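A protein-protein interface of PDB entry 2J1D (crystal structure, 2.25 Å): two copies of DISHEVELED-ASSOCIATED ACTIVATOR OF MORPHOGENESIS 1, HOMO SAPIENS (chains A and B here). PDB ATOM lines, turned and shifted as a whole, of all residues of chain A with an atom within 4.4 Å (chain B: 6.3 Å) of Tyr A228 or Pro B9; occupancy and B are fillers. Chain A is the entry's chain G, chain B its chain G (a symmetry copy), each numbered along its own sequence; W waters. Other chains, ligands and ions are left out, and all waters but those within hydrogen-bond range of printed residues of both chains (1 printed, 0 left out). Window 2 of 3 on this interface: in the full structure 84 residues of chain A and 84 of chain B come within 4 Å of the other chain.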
ATOM      1  N   ALA A 224     -30.321  -1.688  -7.379  1.00  0.00           N
ATOM      2  CA  ALA A 224     -30.880  -2.318  -6.204  1.00  0.00           C
ATOM      3  C   ALA A 224     -30.350  -3.745  -6.051  1.00  0.00           C
ATOM      4  O   ALA A 224     -29.880  -4.108  -4.987  1.00  0.00           O
ATOM      5  CB  ALA A 224     -32.418  -2.312  -6.295  1.00  0.00           C
ATOM      6  N   PHE A 225     -30.412  -4.545  -7.113  1.00  0.00           N
ATOM      7  CA  PHE A 225     -29.937  -5.939  -7.060  1.00  0.00           C
ATOM      8  C   PHE A 225     -28.489  -6.059  -6.600  1.00  0.00           C
ATOM      9  O   PHE A 225     -28.174  -6.870  -5.743  1.00  0.00           O
ATOM     10  CB  PHE A 225     -30.063  -6.617  -8.430  1.00  0.00           C
ATOM     11  CG  PHE A 225     -31.431  -7.190  -8.731  1.00  0.00           C
ATOM     12  CD1 PHE A 225     -32.540  -6.890  -7.971  1.00  0.00           C
ATOM     13  CD2 PHE A 225     -31.601  -8.003  -9.841  1.00  0.00           C
ATOM     14  CE1 PHE A 225     -33.785  -7.427  -8.296  1.00  0.00           C
ATOM     15  CE2 PHE A 225     -32.843  -8.540 -10.159  1.00  0.00           C
ATOM     16  CZ  PHE A 225     -33.925  -8.248  -9.391  1.00  0.00           C
ATOM     17  N   GLY A 226     -27.610  -5.264  -7.194  1.00  0.00           N
ATOM     18  CA  GLY A 226     -26.191  -5.311  -6.868  1.00  0.00           C
ATOM     19  C   GLY A 226     -25.878  -4.802  -5.472  1.00  0.00           C
ATOM     20  O   GLY A 226     -25.028  -5.361  -4.795  1.00  0.00           O
ATOM     21  N   ASN A 227     -26.556  -3.733  -5.055  1.00  0.00           N
ATOM     22  CA  ASN A 227     -26.375  -3.146  -3.721  1.00  0.00           C
ATOM     23  C   ASN A 227     -26.845  -4.078  -2.580  1.00  0.00           C
ATOM     24  O   ASN A 227     -26.319  -4.021  -1.472  1.00  0.00           O
ATOM     25  CB  ASN A 227     -27.070  -1.772  -3.635  1.00  0.00           C
ATOM     26  CG  ASN A 227     -26.174  -0.617  -4.104  1.00  0.00           C
ATOM     27  OD1 ASN A 227     -24.952  -0.732  -4.131  1.00  0.00           O
ATOM     28  ND2 ASN A 227     -26.788   0.506  -4.459  1.00  0.00           N
ATOM     29  N   TYR A 228     -27.821  -4.935  -2.876  1.00  0.00           N
ATOM     30  CA  TYR A 228     -28.283  -5.977  -1.958  1.00  0.00           C
ATOM     31  C   TYR A 228     -27.390  -7.198  -2.002  1.00  0.00           C
ATOM     32  O   TYR A 228     -27.080  -7.771  -0.965  1.00  0.00           O
ATOM     33  CB  TYR A 228     -29.702  -6.416  -2.326  1.00  0.00           C
ATOM     34  CG  TYR A 228     -30.461  -7.203  -1.258  1.00  0.00           C
ATOM     35  CD1 TYR A 228     -30.796  -6.625  -0.042  1.00  0.00           C
ATOM     36  CD2 TYR A 228     -30.886  -8.507  -1.496  1.00  0.00           C
ATOM     37  CE1 TYR A 228     -31.516  -7.334   0.928  1.00  0.00           C
ATOM     38  CE2 TYR A 228     -31.601  -9.220  -0.551  1.00  0.00           C
ATOM     39  CZ  TYR A 228     -31.920  -8.633   0.665  1.00  0.00           C
ATOM     40  OH  TYR A 228     -32.651  -9.350   1.608  1.00  0.00           O
ATOM     41  N   MET A 229     -27.002  -7.613  -3.205  1.00  0.00           N
ATOM     42  CA  MET A 229     -26.254  -8.861  -3.384  1.00  0.00           C
ATOM     43  C   MET A 229     -24.759  -8.713  -3.081  1.00  0.00           C
ATOM     44  O   MET A 229     -24.109  -9.673  -2.659  1.00  0.00           O
ATOM     45  CB  MET A 229     -26.459  -9.401  -4.800  1.00  0.00           C
ATOM     46  CG  MET A 229     -27.881  -9.859  -5.070  1.00  0.00           C
ATOM     47  SD  MET A 229     -28.214 -10.125  -6.815  1.00  0.00           S
ATOM     48  CE  MET A 229     -27.560 -11.779  -7.005  1.00  0.00           C
ATOM     49  N   ASN A 230     -24.220  -7.516  -3.307  1.00  0.00           N
ATOM     50  CA  ASN A 230     -22.792  -7.265  -3.118  1.00  0.00           C
ATOM     51  C   ASN A 230     -22.516  -6.720  -1.725  1.00  0.00           C
ATOM     52  O   ASN A 230     -22.213  -5.542  -1.548  1.00  0.00           O
ATOM     53  CB  ASN A 230     -22.260  -6.311  -4.191  1.00  0.00           C
ATOM     54  CG  ASN A 230     -22.263  -6.940  -5.575  1.00  0.00           C
ATOM     55  OD1 ASN A 230     -22.473  -8.141  -5.723  1.00  0.00           O
ATOM     56  ND2 ASN A 230     -22.048  -6.129  -6.596  1.00  0.00           N
ATOM     57  N   SER B   7     -28.817   4.503   3.100  1.00  0.00           N
ATOM     58  CA  SER B   7     -30.167   3.773   3.150  1.00  0.00           C
ATOM     59  C   SER B   7     -30.610   2.389   2.686  1.00  0.00           C
ATOM     60  O   SER B   7     -31.813   2.106   2.800  1.00  0.00           O
ATOM     61  CB  SER B   7     -31.223   4.607   2.396  1.00  0.00           C
ATOM     62  OG  SER B   7     -32.551   4.124   2.678  1.00  0.00           O
ATOM     63  N   ILE B   8     -29.836   1.395   2.185  1.00  0.00           N
ATOM     64  CA  ILE B   8     -30.406   0.198   1.601  1.00  0.00           C
ATOM     65  C   ILE B   8     -30.400  -0.875   2.720  1.00  0.00           C
ATOM     66  O   ILE B   8     -29.552  -0.805   3.616  1.00  0.00           O
ATOM     67  CB  ILE B   8     -29.544  -0.149   0.358  1.00  0.00           C
ATOM     68  CG1 ILE B   8     -28.200  -0.738   0.783  1.00  0.00           C
ATOM     69  CG2 ILE B   8     -29.323   1.107  -0.502  1.00  0.00           C
ATOM     70  CD1 ILE B   8     -28.153  -2.255   0.704  1.00  0.00           C
ATOM     71  N   PRO B   9     -31.354  -1.841   2.713  1.00  0.00           N
ATOM     72  CA  PRO B   9     -31.312  -2.913   3.715  1.00  0.00           C
ATOM     73  C   PRO B   9     -30.440  -4.058   3.233  1.00  0.00           C
ATOM     74  O   PRO B   9     -30.188  -4.165   2.038  1.00  0.00           O
ATOM     75  CB  PRO B   9     -32.763  -3.374   3.774  1.00  0.00           C
ATOM     76  CG  PRO B   9     -33.236  -3.213   2.384  1.00  0.00           C
ATOM     77  CD  PRO B   9     -32.502  -2.017   1.808  1.00  0.00           C
ATOM     78  N   GLN B  10     -29.990  -4.920   4.136  1.00  0.00           N
ATOM     79  CA  GLN B  10     -29.090  -6.008   3.735  1.00  0.00           C
ATOM     80  C   GLN B  10     -29.658  -7.374   4.162  1.00  0.00           C
ATOM     81  O   GLN B  10     -30.453  -7.448   5.095  1.00  0.00           O
ATOM     82  CB  GLN B  10     -27.663  -5.744   4.250  1.00  0.00           C
ATOM     83  CG  GLN B  10     -27.042  -4.406   3.724  1.00  0.00           C
ATOM     84  CD  GLN B  10     -25.890  -4.586   2.722  1.00  0.00           C
ATOM     85  OE1 GLN B  10     -26.100  -4.851   1.527  1.00  0.00           O
ATOM     86  NE2 GLN B  10     -24.665  -4.413   3.213  1.00  0.00           N
ATOM     87  N   PRO B  11     -29.279  -8.450   3.443  1.00  0.00           N
ATOM     88  CA  PRO B  11     -29.910  -9.771   3.546  1.00  0.00           C
ATOM     89  C   PRO B  11     -29.762 -10.470   4.895  1.00  0.00           C
ATOM     90  O   PRO B  11     -28.885 -10.116   5.686  1.00  0.00           O
ATOM     91  CB  PRO B  11     -29.169 -10.595   2.485  1.00  0.00           C
ATOM     92  CG  PRO B  11     -28.507  -9.621   1.598  1.00  0.00           C
ATOM     93  CD  PRO B  11     -28.189  -8.452   2.449  1.00  0.00           C
ATOM     94  N   THR B  12     -30.612 -11.469   5.137  1.00  0.00           N
ATOM     95  CA  THR B  12     -30.460 -12.343   6.302  1.00  0.00           C
ATOM     96  C   THR B  12     -29.237 -13.258   6.121  1.00  0.00           C
ATOM     97  O   THR B  12     -28.406 -13.355   7.023  1.00  0.00           O
ATOM     98  CB  THR B  12     -31.743 -13.171   6.599  1.00  0.00           C
ATOM     99  OG1 THR B  12     -32.138 -13.892   5.426  1.00  0.00           O
ATOM    100  CG2 THR B  12     -32.887 -12.254   7.044  1.00  0.00           C
ATOM    101  N   LEU B  15     -25.472 -13.480  -0.294  1.00  0.00           N
ATOM    102  CA  LEU B  15     -25.976 -13.724  -1.638  1.00  0.00           C
ATOM    103  C   LEU B  15     -24.837 -13.942  -2.638  1.00  0.00           C
ATOM    104  O   LEU B  15     -23.688 -13.589  -2.384  1.00  0.00           O
ATOM    105  CB  LEU B  15     -26.879 -12.553  -2.086  1.00  0.00           C
ATOM    106  CG  LEU B  15     -28.385 -12.618  -1.758  1.00  0.00           C
ATOM    107  CD1 LEU B  15     -28.671 -13.366  -0.495  1.00  0.00           C
ATOM    108  CD2 LEU B  15     -29.012 -11.233  -1.679  1.00  0.00           C
ATOM    109  N   TRP B  20     -20.715  -6.408 -11.530  1.00  0.00           N
ATOM    110  CA  TRP B  20     -20.880  -5.104 -12.177  1.00  0.00           C
ATOM    111  C   TRP B  20     -19.579  -4.330 -12.120  1.00  0.00           C
ATOM    112  O   TRP B  20     -18.640  -4.776 -11.506  1.00  0.00           O
ATOM    113  CB  TRP B  20     -22.029  -4.301 -11.561  1.00  0.00           C
ATOM    114  CG  TRP B  20     -21.944  -3.973 -10.089  1.00  0.00           C
ATOM    115  CD1 TRP B  20     -20.885  -4.179  -9.227  1.00  0.00           C
ATOM    116  CD2 TRP B  20     -22.961  -3.340  -9.316  1.00  0.00           C
ATOM    117  NE1 TRP B  20     -21.204  -3.721  -7.976  1.00  0.00           N
ATOM    118  CE2 TRP B  20     -22.464  -3.192  -8.003  1.00  0.00           C
ATOM    119  CE3 TRP B  20     -24.249  -2.882  -9.607  1.00  0.00           C
ATOM    120  CZ2 TRP B  20     -23.216  -2.610  -6.987  1.00  0.00           C
ATOM    121  CZ3 TRP B  20     -24.996  -2.304  -8.595  1.00  0.00           C
ATOM    122  CH2 TRP B  20     -24.482  -2.176  -7.304  1.00  0.00           C
ATOM    123  N   THR B  39     -33.557   3.029  -3.571  1.00  0.00           N
ATOM    124  CA  THR B  39     -34.105   2.832  -2.220  1.00  0.00           C
ATOM    125  C   THR B  39     -35.609   2.529  -2.206  1.00  0.00           C
ATOM    126  O   THR B  39     -36.113   1.958  -1.241  1.00  0.00           O
ATOM    127  CB  THR B  39     -33.798   4.015  -1.274  1.00  0.00           C
ATOM    128  OG1 THR B  39     -34.392   5.209  -1.786  1.00  0.00           O
ATOM    129  CG2 THR B  39     -32.296   4.208  -1.138  1.00  0.00           C
ATOM    130  N   PHE B  42     -36.546  -1.527  -2.981  1.00  0.00           N
ATOM    131  CA  PHE B  42     -36.411  -2.490  -1.877  1.00  0.00           C
ATOM    132  C   PHE B  42     -37.741  -2.766  -1.197  1.00  0.00           C
ATOM    133  O   PHE B  42     -38.015  -3.882  -0.756  1.00  0.00           O
ATOM    134  CB  PHE B  42     -35.404  -1.981  -0.839  1.00  0.00           C
ATOM    135  CG  PHE B  42     -34.002  -1.832  -1.379  1.00  0.00           C
ATOM    136  CD1 PHE B  42     -33.344  -0.610  -1.308  1.00  0.00           C
ATOM    137  CD2 PHE B  42     -33.346  -2.912  -1.970  1.00  0.00           C
ATOM    138  CE1 PHE B  42     -32.053  -0.461  -1.813  1.00  0.00           C
ATOM    139  CE2 PHE B  42     -32.061  -2.776  -2.477  1.00  0.00           C
ATOM    140  CZ  PHE B  42     -31.410  -1.546  -2.397  1.00  0.00           C
ATOM    141  N   LEU B  47     -37.853  -9.377  -1.551  1.00  0.00           N
ATOM    142  CA  LEU B  47     -36.445  -9.611  -1.254  1.00  0.00           C
ATOM    143  C   LEU B  47     -36.199 -11.049  -0.783  1.00  0.00           C
ATOM    144  O   LEU B  47     -35.227 -11.680  -1.178  1.00  0.00           O
ATOM    145  CB  LEU B  47     -35.964  -8.607  -0.204  1.00  0.00           C
ATOM    146  CG  LEU B  47     -36.033  -7.137  -0.637  1.00  0.00           C
ATOM    147  CD1 LEU B  47     -35.726  -6.225   0.548  1.00  0.00           C
ATOM    148  CD2 LEU B  47     -35.099  -6.850  -1.816  1.00  0.00           C
ATOM    149  N   GLU B  48     -37.095 -11.562   0.047  1.00  0.00           N
ATOM    150  CA  GLU B  48     -37.057 -12.961   0.493  1.00  0.00           C
ATOM    151  C   GLU B  48     -36.941 -13.956  -0.682  1.00  0.00           C
ATOM    152  O   GLU B  48     -36.209 -14.947  -0.585  1.00  0.00           O
ATOM    153  CB  GLU B  48     -38.306 -13.250   1.336  1.00  0.00           C
ATOM    154  CG  GLU B  48     -38.368 -14.612   2.010  1.00  0.00           C
ATOM    155  CD  GLU B  48     -39.631 -14.782   2.855  1.00  0.00           C
ATOM    156  OE1 GLU B  48     -40.007 -15.943   3.129  1.00  0.00           O
ATOM    157  OE2 GLU B  48     -40.257 -13.767   3.241  1.00  0.00           O
ATOM    158  N   LEU B  50     -35.710 -13.177  -3.707  1.00  0.00           N
ATOM    159  CA  LEU B  50     -34.412 -12.869  -4.323  1.00  0.00           C
ATOM    160  C   LEU B  50     -33.324 -13.674  -3.608  1.00  0.00           C
ATOM    161  O   LEU B  50     -32.499 -14.342  -4.237  1.00  0.00           O
ATOM    162  CB  LEU B  50     -34.125 -11.356  -4.207  1.00  0.00           C
ATOM    163  CG  LEU B  50     -33.216 -10.578  -5.186  1.00  0.00           C
ATOM    164  CD1 LEU B  50     -32.378  -9.599  -4.397  1.00  0.00           C
ATOM    165  CD2 LEU B  50     -32.308 -11.440  -6.036  1.00  0.00           C
ATOM    166  N   GLU B  51     -33.351 -13.602  -2.278  1.00  0.00           N
ATOM    167  CA  GLU B  51     -32.408 -14.315  -1.395  1.00  0.00           C
ATOM    168  C   GLU B  51     -32.415 -15.831  -1.529  1.00  0.00           C
ATOM    169  O   GLU B  51     -31.361 -16.460  -1.520  1.00  0.00           O
ATOM    170  CB  GLU B  51     -32.721 -13.998   0.062  1.00  0.00           C
ATOM    171  CG  GLU B  51     -32.415 -12.583   0.460  1.00  0.00           C
ATOM    172  CD  GLU B  51     -32.329 -12.419   1.957  1.00  0.00           C
ATOM    173  OE1 GLU B  51     -31.606 -13.206   2.607  1.00  0.00           O
ATOM    174  OE2 GLU B  51     -32.977 -11.496   2.487  1.00  0.00           O
HETATM  175  O   HOH W   1     -24.350 -10.571  -0.213  1.00  0.00           O
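The side-chain amide oxygen of Gln B10 sits close to the backbone carbonyl oxygen of Asn A227 (3.1 Å).
ND2 of Asn A230 lies close to NE1 of Trp B20 (2.9 Å).
OH of Tyr A228 lies close to OE2 of Glu B51 (2.3 Å).
Among the printed residues, merely in contact across the chains: Tyr A228 with Pro B9, Tyr A228 with Leu B15, Asn A227 with Ile B8, Tyr A228 with Pro B11, Asn A227 with Trp B20, Tyr A228 with Leu B50, Gly A226 with Trp B20, Ala A224 with Phe B42, Tyr A228 with Gln B10, Met A229 with Leu B15 and Tyr A228 with Leu B47.
Water W1 bridges the backbone carbonyl oxygen (O) of Met A229 (2.6 Å) and the backbone NH (N) of Leu B15 (3.1 Å).
Hydrophobic or aromatic side chains of chain B that line the printed part of chain A: Ile B8, Pro B11, Leu B15, Trp B20, Phe B42, Leu B47 and Leu B50.
Along chain B the printed residues that touch a printed residue of chain A span positions 8 to 51.
Of the 7 printed residues of chain A, 6 touch a printed residue of chain B.
Printed residues of chain A that touch a printed residue of chain B: Ala A224, Gly A226, Asn A227, Tyr A228, Met A229 and Asn A230.
Hydrophobic or aromatic side chains of chain A within 4 Å of the printed part of chain B: Ala A224, Tyr A228 and Met A229.
Among the printed residues, no Asp or Glu carboxylate lies within 4 Å of a Lys or Arg side-chain nitrogen of the other chain.
No position is printed for both chains.
Of the 14 pairs that touch across the chains among the printed residues, none has its exchanged pair printed and touching as well.
The side-chain carboxylate (OE1) of Glu B51 is in hydrogen-bond range of the side-chain hydroxyl (OG1) of Thr B12 (2.9 Å).
Tyr A228 touches just these residues of chain B: Pro B9 (3.3 Å), Gln B10 (3.7 Å), Pro B11 (3.4 Å), Leu B15 (3.3 Å), Leu B47 (3.8 Å), Leu B50 (3.4 Å) and Glu B51 (2.3 Å).
Printed residues of chain A within 4 Å of Ile B8: Asn A227.
Of chain A, only Tyr A228 comes within 4 Å of Pro B9.
Thr B12 touches none of the printed residues of chain A.
Of the printed residues of chain A, Leu B15 touches Tyr A228 and Met A229.
Thr B39 touches none of the printed residues of chain A.
Printed residues of chain A within 4 Å of Leu B47: Tyr A228.
Of the printed residues of chain A, Leu B50 touches Tyr A228.
The nearest residue of chain B that does not touch Tyr A228 is Phe B42 (4.3 Å).
The nearest printed residue of chain A that does not touch Pro B9 is Asn A227 (5.2 Å).
The nearest printed residue of chain A that does not touch Trp B20 is Ala A224 (5.5 Å).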
